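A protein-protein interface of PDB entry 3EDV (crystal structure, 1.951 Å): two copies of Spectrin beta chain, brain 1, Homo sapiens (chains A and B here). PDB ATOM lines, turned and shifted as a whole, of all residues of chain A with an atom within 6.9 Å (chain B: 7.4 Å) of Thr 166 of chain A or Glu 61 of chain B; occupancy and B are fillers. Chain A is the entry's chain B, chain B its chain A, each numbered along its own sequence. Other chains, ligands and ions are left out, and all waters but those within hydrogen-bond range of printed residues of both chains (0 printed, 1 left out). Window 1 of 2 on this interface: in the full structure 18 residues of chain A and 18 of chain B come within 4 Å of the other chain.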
ATOM      1  N   ILE A 125      11.204  34.479   1.762  1.00  0.00           N
ATOM      2  CA  ILE A 125      12.593  34.096   2.068  1.00  0.00           C
ATOM      3  C   ILE A 125      13.147  35.010   3.173  1.00  0.00           C
ATOM      4  O   ILE A 125      13.795  34.548   4.148  1.00  0.00           O
ATOM      5  CB  ILE A 125      13.492  34.108   0.791  1.00  0.00           C
ATOM      6  CG1 ILE A 125      13.000  33.048  -0.204  1.00  0.00           C
ATOM      7  CG2 ILE A 125      14.927  33.844   1.157  1.00  0.00           C
ATOM      8  CD1 ILE A 125      13.655  33.119  -1.589  1.00  0.00           C
ATOM      9  N   ARG A 128      11.668  33.933   6.530  1.00  0.00           N
ATOM     10  CA  ARG A 128      12.319  32.680   6.935  1.00  0.00           C
ATOM     11  C   ARG A 128      13.763  32.886   7.419  1.00  0.00           C
ATOM     12  O   ARG A 128      14.179  32.308   8.409  1.00  0.00           O
ATOM     13  CB  ARG A 128      12.284  31.658   5.794  1.00  0.00           C
ATOM     14  CG  ARG A 128      10.914  31.013   5.590  1.00  0.00           C
ATOM     15  CD  ARG A 128      10.911  30.271   4.271  1.00  0.00           C
ATOM     16  NE  ARG A 128       9.580  29.828   3.882  1.00  0.00           N
ATOM     17  CZ  ARG A 128       9.342  28.955   2.908  1.00  0.00           C
ATOM     18  NH1 ARG A 128      10.355  28.441   2.216  1.00  0.00           N
ATOM     19  NH2 ARG A 128       8.093  28.595   2.613  1.00  0.00           N
ATOM     20  N   ILE A 161      20.126  25.254   7.337  1.00  0.00           N
ATOM     21  CA  ILE A 161      19.925  26.530   6.626  1.00  0.00           C
ATOM     22  C   ILE A 161      20.335  26.524   5.132  1.00  0.00           C
ATOM     23  O   ILE A 161      19.927  27.405   4.364  1.00  0.00           O
ATOM     24  CB  ILE A 161      20.524  27.750   7.358  1.00  0.00           C
ATOM     25  CG1 ILE A 161      22.037  27.691   7.420  1.00  0.00           C
ATOM     26  CG2 ILE A 161      20.010  27.822   8.803  1.00  0.00           C
ATOM     27  CD1 ILE A 161      22.658  29.008   7.927  1.00  0.00           C
ATOM     28  N   GLN A 162      21.114  25.527   4.715  1.00  0.00           N
ATOM     29  CA  GLN A 162      21.487  25.423   3.281  1.00  0.00           C
ATOM     30  C   GLN A 162      20.301  25.372   2.317  1.00  0.00           C
ATOM     31  O   GLN A 162      20.404  25.879   1.173  1.00  0.00           O
ATOM     32  CB  GLN A 162      22.537  24.327   3.022  1.00  0.00           C
ATOM     33  CG  GLN A 162      23.914  24.747   3.593  1.00  0.00           C
ATOM     34  CD  GLN A 162      24.393  26.073   3.028  1.00  0.00           C
ATOM     35  OE1 GLN A 162      24.363  26.284   1.816  1.00  0.00           O
ATOM     36  NE2 GLN A 162      24.839  26.979   3.907  1.00  0.00           N
ATOM     37  N   ALA A 163      19.174  24.845   2.795  1.00  0.00           N
ATOM     38  CA  ALA A 163      17.924  24.872   2.024  1.00  0.00           C
ATOM     39  C   ALA A 163      17.467  26.309   1.753  1.00  0.00           C
ATOM     40  O   ALA A 163      16.992  26.624   0.657  1.00  0.00           O
ATOM     41  CB  ALA A 163      16.825  24.071   2.756  1.00  0.00           C
ATOM     42  N   LEU A 164      17.620  27.194   2.756  1.00  0.00           N
ATOM     43  CA  LEU A 164      17.274  28.615   2.577  1.00  0.00           C
ATOM     44  C   LEU A 164      18.252  29.267   1.647  1.00  0.00           C
ATOM     45  O   LEU A 164      17.881  30.122   0.861  1.00  0.00           O
ATOM     46  CB  LEU A 164      17.306  29.389   3.897  1.00  0.00           C
ATOM     47  CG  LEU A 164      16.245  29.207   4.958  1.00  0.00           C
ATOM     48  CD1 LEU A 164      16.403  30.386   5.936  1.00  0.00           C
ATOM     49  CD2 LEU A 164      14.842  29.154   4.350  1.00  0.00           C
ATOM     50  N   GLY A 165      19.522  28.895   1.774  1.00  0.00           N
ATOM     51  CA  GLY A 165      20.533  29.353   0.845  1.00  0.00           C
ATOM     52  C   GLY A 165      20.122  29.051  -0.586  1.00  0.00           C
ATOM     53  O   GLY A 165      20.212  29.931  -1.482  1.00  0.00           O
ATOM     54  N   THR A 166      19.692  27.811  -0.813  1.00  0.00           N
ATOM     55  CA  THR A 166      19.228  27.429  -2.158  1.00  0.00           C
ATOM     56  C   THR A 166      18.109  28.311  -2.628  1.00  0.00           C
ATOM     57  O   THR A 166      18.099  28.684  -3.814  1.00  0.00           O
ATOM     58  CB  THR A 166      18.792  25.956  -2.235  1.00  0.00           C
ATOM     59  OG1 THR A 166      19.918  25.131  -1.904  1.00  0.00           O
ATOM     60  CG2 THR A 166      18.293  25.611  -3.633  1.00  0.00           C
ATOM     61  N   GLN A 167      17.179  28.645  -1.723  1.00  0.00           N
ATOM     62  CA  GLN A 167      16.032  29.493  -2.066  1.00  0.00           C
ATOM     63  C   GLN A 167      16.518  30.933  -2.358  1.00  0.00           C
ATOM     64  O   GLN A 167      16.052  31.574  -3.296  1.00  0.00           O
ATOM     65  CB  GLN A 167      15.013  29.504  -0.928  1.00  0.00           C
ATOM     66  CG  GLN A 167      14.225  28.194  -0.782  1.00  0.00           C
ATOM     67  CD  GLN A 167      13.503  28.099   0.545  1.00  0.00           C
ATOM     68  OE1 GLN A 167      12.769  29.003   0.944  1.00  0.00           O
ATOM     69  NE2 GLN A 167      13.718  27.003   1.243  1.00  0.00           N
ATOM     70  N   VAL A 168      17.484  31.409  -1.559  1.00  0.00           N
ATOM     71  CA  VAL A 168      18.150  32.670  -1.855  1.00  0.00           C
ATOM     72  C   VAL A 168      18.764  32.704  -3.272  1.00  0.00           C
ATOM     73  O   VAL A 168      18.493  33.645  -4.024  1.00  0.00           O
ATOM     74  CB  VAL A 168      19.160  33.079  -0.731  1.00  0.00           C
ATOM     75  CG1 VAL A 168      20.006  34.313  -1.170  1.00  0.00           C
ATOM     76  CG2 VAL A 168      18.363  33.440   0.509  1.00  0.00           C
ATOM     77  N   ARG A 169      19.578  31.705  -3.634  1.00  0.00           N
ATOM     78  CA  ARG A 169      20.186  31.661  -4.978  1.00  0.00           C
ATOM     79  C   ARG A 169      19.125  31.644  -6.082  1.00  0.00           C
ATOM     80  O   ARG A 169      19.273  32.362  -7.073  1.00  0.00           O
ATOM     81  CB  ARG A 169      21.166  30.483  -5.116  1.00  0.00           C
ATOM     82  CG  ARG A 169      22.409  30.622  -4.195  1.00  0.00           C
ATOM     83  CD  ARG A 169      23.427  29.490  -4.418  1.00  0.00           C
ATOM     84  NE  ARG A 169      22.950  28.156  -4.014  1.00  0.00           N
ATOM     85  CZ  ARG A 169      22.943  27.671  -2.773  1.00  0.00           C
ATOM     86  NH1 ARG A 169      23.376  28.378  -1.743  1.00  0.00           N
ATOM     87  NH2 ARG A 169      22.500  26.443  -2.556  1.00  0.00           N
ATOM     88  N   GLN A 170      18.048  30.863  -5.899  1.00  0.00           N
ATOM     89  CA  GLN A 170      16.870  30.903  -6.807  1.00  0.00           C
ATOM     90  C   GLN A 170      16.265  32.306  -6.974  1.00  0.00           C
ATOM     91  O   GLN A 170      16.006  32.747  -8.107  1.00  0.00           O
ATOM     92  CB  GLN A 170      15.766  29.925  -6.364  1.00  0.00           C
ATOM     93  CG  GLN A 170      14.570  29.813  -7.373  1.00  0.00           C
ATOM     94  CD  GLN A 170      14.998  29.430  -8.806  1.00  0.00           C
ATOM     95  OE1 GLN A 170      15.711  28.449  -9.017  1.00  0.00           O
ATOM     96  NE2 GLN A 170      14.564  30.220  -9.786  1.00  0.00           N
ATOM     97  N   LEU A 171      16.053  32.997  -5.856  1.00  0.00           N
ATOM     98  CA  LEU A 171      15.593  34.385  -5.879  1.00  0.00           C
ATOM     99  C   LEU A 171      16.536  35.272  -6.712  1.00  0.00           C
ATOM    100  O   LEU A 171      16.087  36.129  -7.453  1.00  0.00           O
ATOM    101  CB  LEU A 171      15.449  34.952  -4.464  1.00  0.00           C
ATOM    102  CG  LEU A 171      14.708  36.289  -4.318  1.00  0.00           C
ATOM    103  CD1 LEU A 171      13.212  36.141  -4.630  1.00  0.00           C
ATOM    104  CD2 LEU A 171      14.940  36.917  -2.957  1.00  0.00           C
ATOM    105  N   GLU A 173      18.474  34.288  -9.221  1.00  0.00           N
ATOM    106  CA  GLU A 173      18.230  34.005 -10.647  1.00  0.00           C
ATOM    107  C   GLU A 173      16.957  34.635 -11.187  1.00  0.00           C
ATOM    108  O   GLU A 173      16.961  35.147 -12.295  1.00  0.00           O
ATOM    109  CB  GLU A 173      18.234  32.506 -10.957  1.00  0.00           C
ATOM    110  CG  GLU A 173      19.610  31.849 -10.832  1.00  0.00           C
ATOM    111  CD  GLU A 173      19.508  30.345 -10.769  1.00  0.00           C
ATOM    112  OE1 GLU A 173      18.858  29.762 -11.675  1.00  0.00           O
ATOM    113  OE2 GLU A 173      20.062  29.757  -9.812  1.00  0.00           O
ATOM    114  N   TRP A 201      20.466  37.340   4.610  1.00  0.00           N
ATOM    115  CA  TRP A 201      21.204  36.089   4.442  1.00  0.00           C
ATOM    116  C   TRP A 201      22.670  36.195   4.902  1.00  0.00           C
ATOM    117  O   TRP A 201      23.091  35.382   5.706  1.00  0.00           O
ATOM    118  CB  TRP A 201      21.112  35.590   2.996  1.00  0.00           C
ATOM    119  CG  TRP A 201      21.800  34.266   2.736  1.00  0.00           C
ATOM    120  CD1 TRP A 201      22.872  34.055   1.914  1.00  0.00           C
ATOM    121  CD2 TRP A 201      21.489  32.990   3.325  1.00  0.00           C
ATOM    122  NE1 TRP A 201      23.220  32.727   1.927  1.00  0.00           N
ATOM    123  CE2 TRP A 201      22.394  32.054   2.790  1.00  0.00           C
ATOM    124  CE3 TRP A 201      20.507  32.542   4.229  1.00  0.00           C
ATOM    125  CZ2 TRP A 201      22.365  30.691   3.138  1.00  0.00           C
ATOM    126  CZ3 TRP A 201      20.482  31.178   4.571  1.00  0.00           C
ATOM    127  CH2 TRP A 201      21.400  30.281   4.031  1.00  0.00           C
ATOM    128  N   LEU B  18      17.609  11.515  -0.328  1.00  0.00           N
ATOM    129  CA  LEU B  18      17.274  12.082  -1.628  1.00  0.00           C
ATOM    130  C   LEU B  18      17.247  11.022  -2.722  1.00  0.00           C
ATOM    131  O   LEU B  18      16.360  11.028  -3.583  1.00  0.00           O
ATOM    132  CB  LEU B  18      18.197  13.248  -1.998  1.00  0.00           C
ATOM    133  CG  LEU B  18      17.842  14.048  -3.261  1.00  0.00           C
ATOM    134  CD1 LEU B  18      16.343  14.436  -3.320  1.00  0.00           C
ATOM    135  CD2 LEU B  18      18.720  15.284  -3.370  1.00  0.00           C
ATOM    136  N   THR B  55       7.461  17.395  -8.922  1.00  0.00           N
ATOM    137  CA  THR B  55       8.719  16.656  -8.853  1.00  0.00           C
ATOM    138  C   THR B  55       9.914  17.513  -9.234  1.00  0.00           C
ATOM    139  O   THR B  55      10.913  17.498  -8.527  1.00  0.00           O
ATOM    140  CB  THR B  55       8.687  15.374  -9.721  1.00  0.00           C
ATOM    141  OG1 THR B  55       7.625  14.544  -9.246  1.00  0.00           O
ATOM    142  CG2 THR B  55      10.016  14.600  -9.608  1.00  0.00           C
ATOM    143  N   GLY B  56       9.797  18.248 -10.343  1.00  0.00           N
ATOM    144  CA  GLY B  56      10.844  19.136 -10.828  1.00  0.00           C
ATOM    145  C   GLY B  56      11.158  20.264  -9.866  1.00  0.00           C
ATOM    146  O   GLY B  56      12.319  20.598  -9.631  1.00  0.00           O
ATOM    147  N   ASN B  57      10.120  20.846  -9.289  1.00  0.00           N
ATOM    148  CA  ASN B  57      10.299  21.971  -8.374  1.00  0.00           C
ATOM    149  C   ASN B  57      10.877  21.553  -7.023  1.00  0.00           C
ATOM    150  O   ASN B  57      11.841  22.175  -6.559  1.00  0.00           O
ATOM    151  CB  ASN B  57       8.993  22.750  -8.203  1.00  0.00           C
ATOM    152  CG  ASN B  57       8.625  23.553  -9.452  1.00  0.00           C
ATOM    153  OD1 ASN B  57       9.498  23.998 -10.215  1.00  0.00           O
ATOM    154  ND2 ASN B  57       7.330  23.746  -9.662  1.00  0.00           N
ATOM    155  N   ILE B  58      10.287  20.520  -6.411  1.00  0.00           N
ATOM    156  CA  ILE B  58      10.768  19.956  -5.136  1.00  0.00           C
ATOM    157  C   ILE B  58      12.175  19.353  -5.336  1.00  0.00           C
ATOM    158  O   ILE B  58      13.146  19.677  -4.602  1.00  0.00           O
ATOM    159  CB  ILE B  58       9.757  18.894  -4.554  1.00  0.00           C
ATOM    160  CG1 ILE B  58       8.427  19.550  -4.200  1.00  0.00           C
ATOM    161  CG2 ILE B  58      10.355  18.158  -3.312  1.00  0.00           C
ATOM    162  CD1 ILE B  58       7.240  18.556  -4.074  1.00  0.00           C
ATOM    163  N   GLY B  59      12.286  18.528  -6.378  1.00  0.00           N
ATOM    164  CA  GLY B  59      13.531  17.849  -6.702  1.00  0.00           C
ATOM    165  C   GLY B  59      14.730  18.766  -6.933  1.00  0.00           C
ATOM    166  O   GLY B  59      15.820  18.503  -6.416  1.00  0.00           O
ATOM    167  N   GLN B  60      14.541  19.818  -7.719  1.00  0.00           N
ATOM    168  CA  GLN B  60      15.681  20.631  -8.121  1.00  0.00           C
ATOM    169  C   GLN B  60      16.288  21.316  -6.913  1.00  0.00           C
ATOM    170  O   GLN B  60      17.486  21.370  -6.784  1.00  0.00           O
ATOM    171  CB  GLN B  60      15.348  21.644  -9.234  1.00  0.00           C
ATOM    172  CG  GLN B  60      16.593  22.262  -9.896  1.00  0.00           C
ATOM    173  CD  GLN B  60      17.487  21.205 -10.501  1.00  0.00           C
ATOM    174  OE1 GLN B  60      17.075  20.463 -11.385  1.00  0.00           O
ATOM    175  NE2 GLN B  60      18.705  21.121 -10.023  1.00  0.00           N
ATOM    176  N   GLU B  61      15.437  21.837  -6.036  1.00  0.00           N
ATOM    177  CA  GLU B  61      15.899  22.523  -4.835  1.00  0.00           C
ATOM    178  C   GLU B  61      16.704  21.587  -3.940  1.00  0.00           C
ATOM    179  O   GLU B  61      17.732  21.975  -3.385  1.00  0.00           O
ATOM    180  CB  GLU B  61      14.716  23.104  -4.059  1.00  0.00           C
ATOM    181  CG  GLU B  61      15.114  23.974  -2.878  1.00  0.00           C
ATOM    182  CD  GLU B  61      13.921  24.618  -2.201  1.00  0.00           C
ATOM    183  OE1 GLU B  61      13.161  25.335  -2.885  1.00  0.00           O
ATOM    184  OE2 GLU B  61      13.742  24.407  -0.982  1.00  0.00           O
ATOM    185  N   ARG B  62      16.230  20.353  -3.804  1.00  0.00           N
ATOM    186  CA  ARG B  62      16.876  19.375  -2.938  1.00  0.00           C
ATOM    187  C   ARG B  62      18.225  18.942  -3.505  1.00  0.00           C
ATOM    188  O   ARG B  62      19.224  18.898  -2.787  1.00  0.00           O
ATOM    189  CB  ARG B  62      15.973  18.155  -2.741  1.00  0.00           C
ATOM    190  CG  ARG B  62      14.793  18.400  -1.815  1.00  0.00           C
ATOM    191  CD  ARG B  62      14.088  17.100  -1.464  1.00  0.00           C
ATOM    192  NE  ARG B  62      14.922  16.229  -0.641  1.00  0.00           N
ATOM    193  CZ  ARG B  62      14.529  15.053  -0.161  1.00  0.00           C
ATOM    194  NH1 ARG B  62      13.309  14.603  -0.422  1.00  0.00           N
ATOM    195  NH2 ARG B  62      15.355  14.327   0.579  1.00  0.00           N
ATOM    196  N   VAL B  63      18.245  18.625  -4.795  1.00  0.00           N
ATOM    197  CA  VAL B  63      19.489  18.314  -5.488  1.00  0.00           C
ATOM    198  C   VAL B  63      20.507  19.438  -5.323  1.00  0.00           C
ATOM    199  O   VAL B  63      21.649  19.201  -4.930  1.00  0.00           O
ATOM    200  CB  VAL B  63      19.252  18.066  -6.989  1.00  0.00           C
ATOM    201  CG1 VAL B  63      20.579  17.895  -7.714  1.00  0.00           C
ATOM    202  CG2 VAL B  63      18.365  16.847  -7.191  1.00  0.00           C
ATOM    203  N   ASP B  64      20.085  20.661  -5.626  1.00  0.00           N
ATOM    204  CA  ASP B  64      20.965  21.820  -5.531  1.00  0.00           C
ATOM    205  C   ASP B  64      21.464  22.018  -4.103  1.00  0.00           C
ATOM    206  O   ASP B  64      22.627  22.359  -3.883  1.00  0.00           O
ATOM    207  CB  ASP B  64      20.245  23.081  -6.016  1.00  0.00           C
ATOM    208  CG  ASP B  64      20.108  23.128  -7.525  1.00  0.00           C
ATOM    209  OD1 ASP B  64      20.860  22.409  -8.215  1.00  0.00           O
ATOM    210  OD2 ASP B  64      19.248  23.886  -8.021  1.00  0.00           O
ATOM    211  N   THR B  65      20.578  21.802  -3.136  1.00  0.00           N
ATOM    212  CA  THR B  65      20.940  21.901  -1.728  1.00  0.00           C
ATOM    213  C   THR B  65      22.022  20.890  -1.364  1.00  0.00           C
ATOM    214  O   THR B  65      23.046  21.243  -0.780  1.00  0.00           O
ATOM    215  CB  THR B  65      19.720  21.687  -0.814  1.00  0.00           C
ATOM    216  OG1 THR B  65      18.749  22.711  -1.058  1.00  0.00           O
ATOM    217  CG2 THR B  65      20.136  21.727   0.648  1.00  0.00           C
ATOM    218  N   VAL B  66      21.786  19.629  -1.713  1.00  0.00           N
ATOM    219  CA  VAL B  66      22.748  18.565  -1.439  1.00  0.00           C
ATOM    220  C   VAL B  66      24.097  18.788  -2.182  1.00  0.00           C
ATOM    221  O   VAL B  66      25.154  18.497  -1.609  1.00  0.00           O
ATOM    222  CB  VAL B  66      22.114  17.159  -1.709  1.00  0.00           C
ATOM    223  CG1 VAL B  66      23.116  16.051  -1.473  1.00  0.00           C
ATOM    224  CG2 VAL B  66      20.894  16.950  -0.814  1.00  0.00           C
ATOM    225  N   ASN B  67      24.066  19.289  -3.434  1.00  0.00           N
ATOM    226  CA  ASN B  67      25.314  19.595  -4.169  1.00  0.00           C
ATOM    227  C   ASN B  67      26.167  20.625  -3.463  1.00  0.00           C
ATOM    228  O   ASN B  67      27.390  20.464  -3.383  1.00  0.00           O
ATOM    229  CB  ASN B  67      25.063  20.115  -5.609  1.00  0.00           C
ATOM    230  CG  ASN B  67      24.955  18.987  -6.625  1.00  0.00           C
ATOM    231  OD1 ASN B  67      25.876  18.744  -7.395  1.00  0.00           O
ATOM    232  ND2 ASN B  67      23.820  18.307  -6.637  1.00  0.00           N
ATOM    233  N   HIS B  68      25.515  21.704  -3.016  1.00  0.00           N
ATOM    234  CA  HIS B  68      26.161  22.756  -2.245  1.00  0.00           C
ATOM    235  C   HIS B  68      26.881  22.191  -1.020  1.00  0.00           C
ATOM    236  O   HIS B  68      28.065  22.482  -0.805  1.00  0.00           O
ATOM    237  CB  HIS B  68      25.159  23.835  -1.823  1.00  0.00           C
ATOM    238  CG  HIS B  68      25.808  25.126  -1.422  1.00  0.00           C
ATOM    239  ND1 HIS B  68      26.129  25.426  -0.112  1.00  0.00           N
ATOM    240  CD2 HIS B  68      26.189  26.200  -2.159  1.00  0.00           C
ATOM    241  CE1 HIS B  68      26.691  26.623  -0.062  1.00  0.00           C
ATOM    242  NE2 HIS B  68      26.738  27.116  -1.289  1.00  0.00           N
ATOM    243  N   TRP B  95      19.301  12.153 -10.774  1.00  0.00           N
ATOM    244  CA  TRP B  95      18.414  13.293 -11.025  1.00  0.00           C
ATOM    245  C   TRP B  95      18.196  13.601 -12.512  1.00  0.00           C
ATOM    246  O   TRP B  95      17.053  13.777 -12.958  1.00  0.00           O
ATOM    247  CB  TRP B  95      18.956  14.542 -10.347  1.00  0.00           C
ATOM    248  CG  TRP B  95      18.080  15.762 -10.564  1.00  0.00           C
ATOM    249  CD1 TRP B  95      18.483  16.971 -11.057  1.00  0.00           C
ATOM    250  CD2 TRP B  95      16.679  15.888 -10.282  1.00  0.00           C
ATOM    251  NE1 TRP B  95      17.440  17.848 -11.070  1.00  0.00           N
ATOM    252  CE2 TRP B  95      16.312  17.217 -10.612  1.00  0.00           C
ATOM    253  CE3 TRP B  95      15.693  15.015  -9.771  1.00  0.00           C
ATOM    254  CZ2 TRP B  95      14.996  17.698 -10.469  1.00  0.00           C
ATOM    255  CZ3 TRP B  95      14.365  15.496  -9.637  1.00  0.00           C
ATOM    256  CH2 TRP B  95      14.045  16.826  -9.990  1.00  0.00           C
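The side-chain carboxylate (OE2) of Glu 61 of chain B is in hydrogen-bond range of the side-chain amide nitrogen (NE2) of Gln 167 of chain A. OG1 of Thr 166 of chain A lies within hydrogen-bond range of OG1 of Thr 65 of chain B (2.8 Å). A ring nitrogen (ND1) of His 68 of chain B sits at hydrogen-bond distance from the side-chain amide oxygen (OE1) of Gln 162 of chain A, 2.8 Å away.
The side-chain amide nitrogen of Gln 60 of chain B is in hydrogen-bond range of the side-chain carboxylate of Asp 64 of chain B (3.1 Å). OG1 of Thr 65 of chain B sits at hydrogen-bond distance from O of Glu 61 of chain B (2.6 Å). The guanidinium group (NH1) of Arg 128 of chain A lies within hydrogen-bond range of the side-chain amide oxygen (OE1) of Gln 167 of chain A (2.8 Å). OG1 of Thr 166 of chain A lies within hydrogen-bond range of O of Gln 162 of chain A, 3.2 Å away. The backbone carbonyl oxygen of Ala 163 of chain A is in hydrogen-bond range of the side-chain amide nitrogen of Gln 167 of chain A, at 3.3 Å. The guanidinium group (NH2) of Arg 169 of chain A lies within hydrogen-bond range of the side-chain hydroxyl (OG1) of Thr 166 of chain A.
Ala 163 of chain A touches Thr 65 of chain B (CA to OG1, 3.9 Å). Glu 61 of chain B touches Thr 166 of chain A (CG to CG2, 3.7 Å). Thr 166 of chain A touches Asp 64 of chain B. Arg 169 of chain A touches His 68 of chain B (NH1 to CD2, 3.6 Å).
Printed residues of chain B within 4 Å of Gln 162 of chain A: His 68 (2.8 Å). Of the printed residues of chain B, Ala 163 of chain A touches Thr 65. No residue of chain B comes within 4 Å of Gly 165 of chain A. Printed residues of chain B within 4 Å of Thr 166 of chain A: Glu 61, Asp 64 and Thr 65. Glu 61 of chain B touches just these residues of chain A: Thr 166 (3.7 Å) and Gln 167 (3.4 Å). Printed residues of chain A within 4 Å of Asp 64 of chain B: Thr 166 (3.99 Å). Printed residues of chain A within 4 Å of Thr 65 of chain B: Ala 163 (3.9 Å) and Thr 166 (2.8 Å). Printed residues of chain A within 4 Å of His 68 of chain B: Gln 162 and Arg 169. The nearest residue of chain A that does not touch Glu 61 of chain B is Ala 163 of chain A (4.3 Å). The nearest printed residue of chain B that does not touch Gln 162 of chain A is Thr 65 of chain B (4.01 Å).
Hydrophobic or aromatic side chains of chain B within 4 Å of the printed part of chain A: His 68. Among the printed residues, 7 pairs touch across the chains. Among the printed residues, no Asp or Glu carboxylate lies within 4 Å of a Lys or Arg side-chain nitrogen of the other chain.
No position is printed for both chains. Of the 7 pairs that touch across the chains among the printed residues, none has its exchanged pair printed and touching as well.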
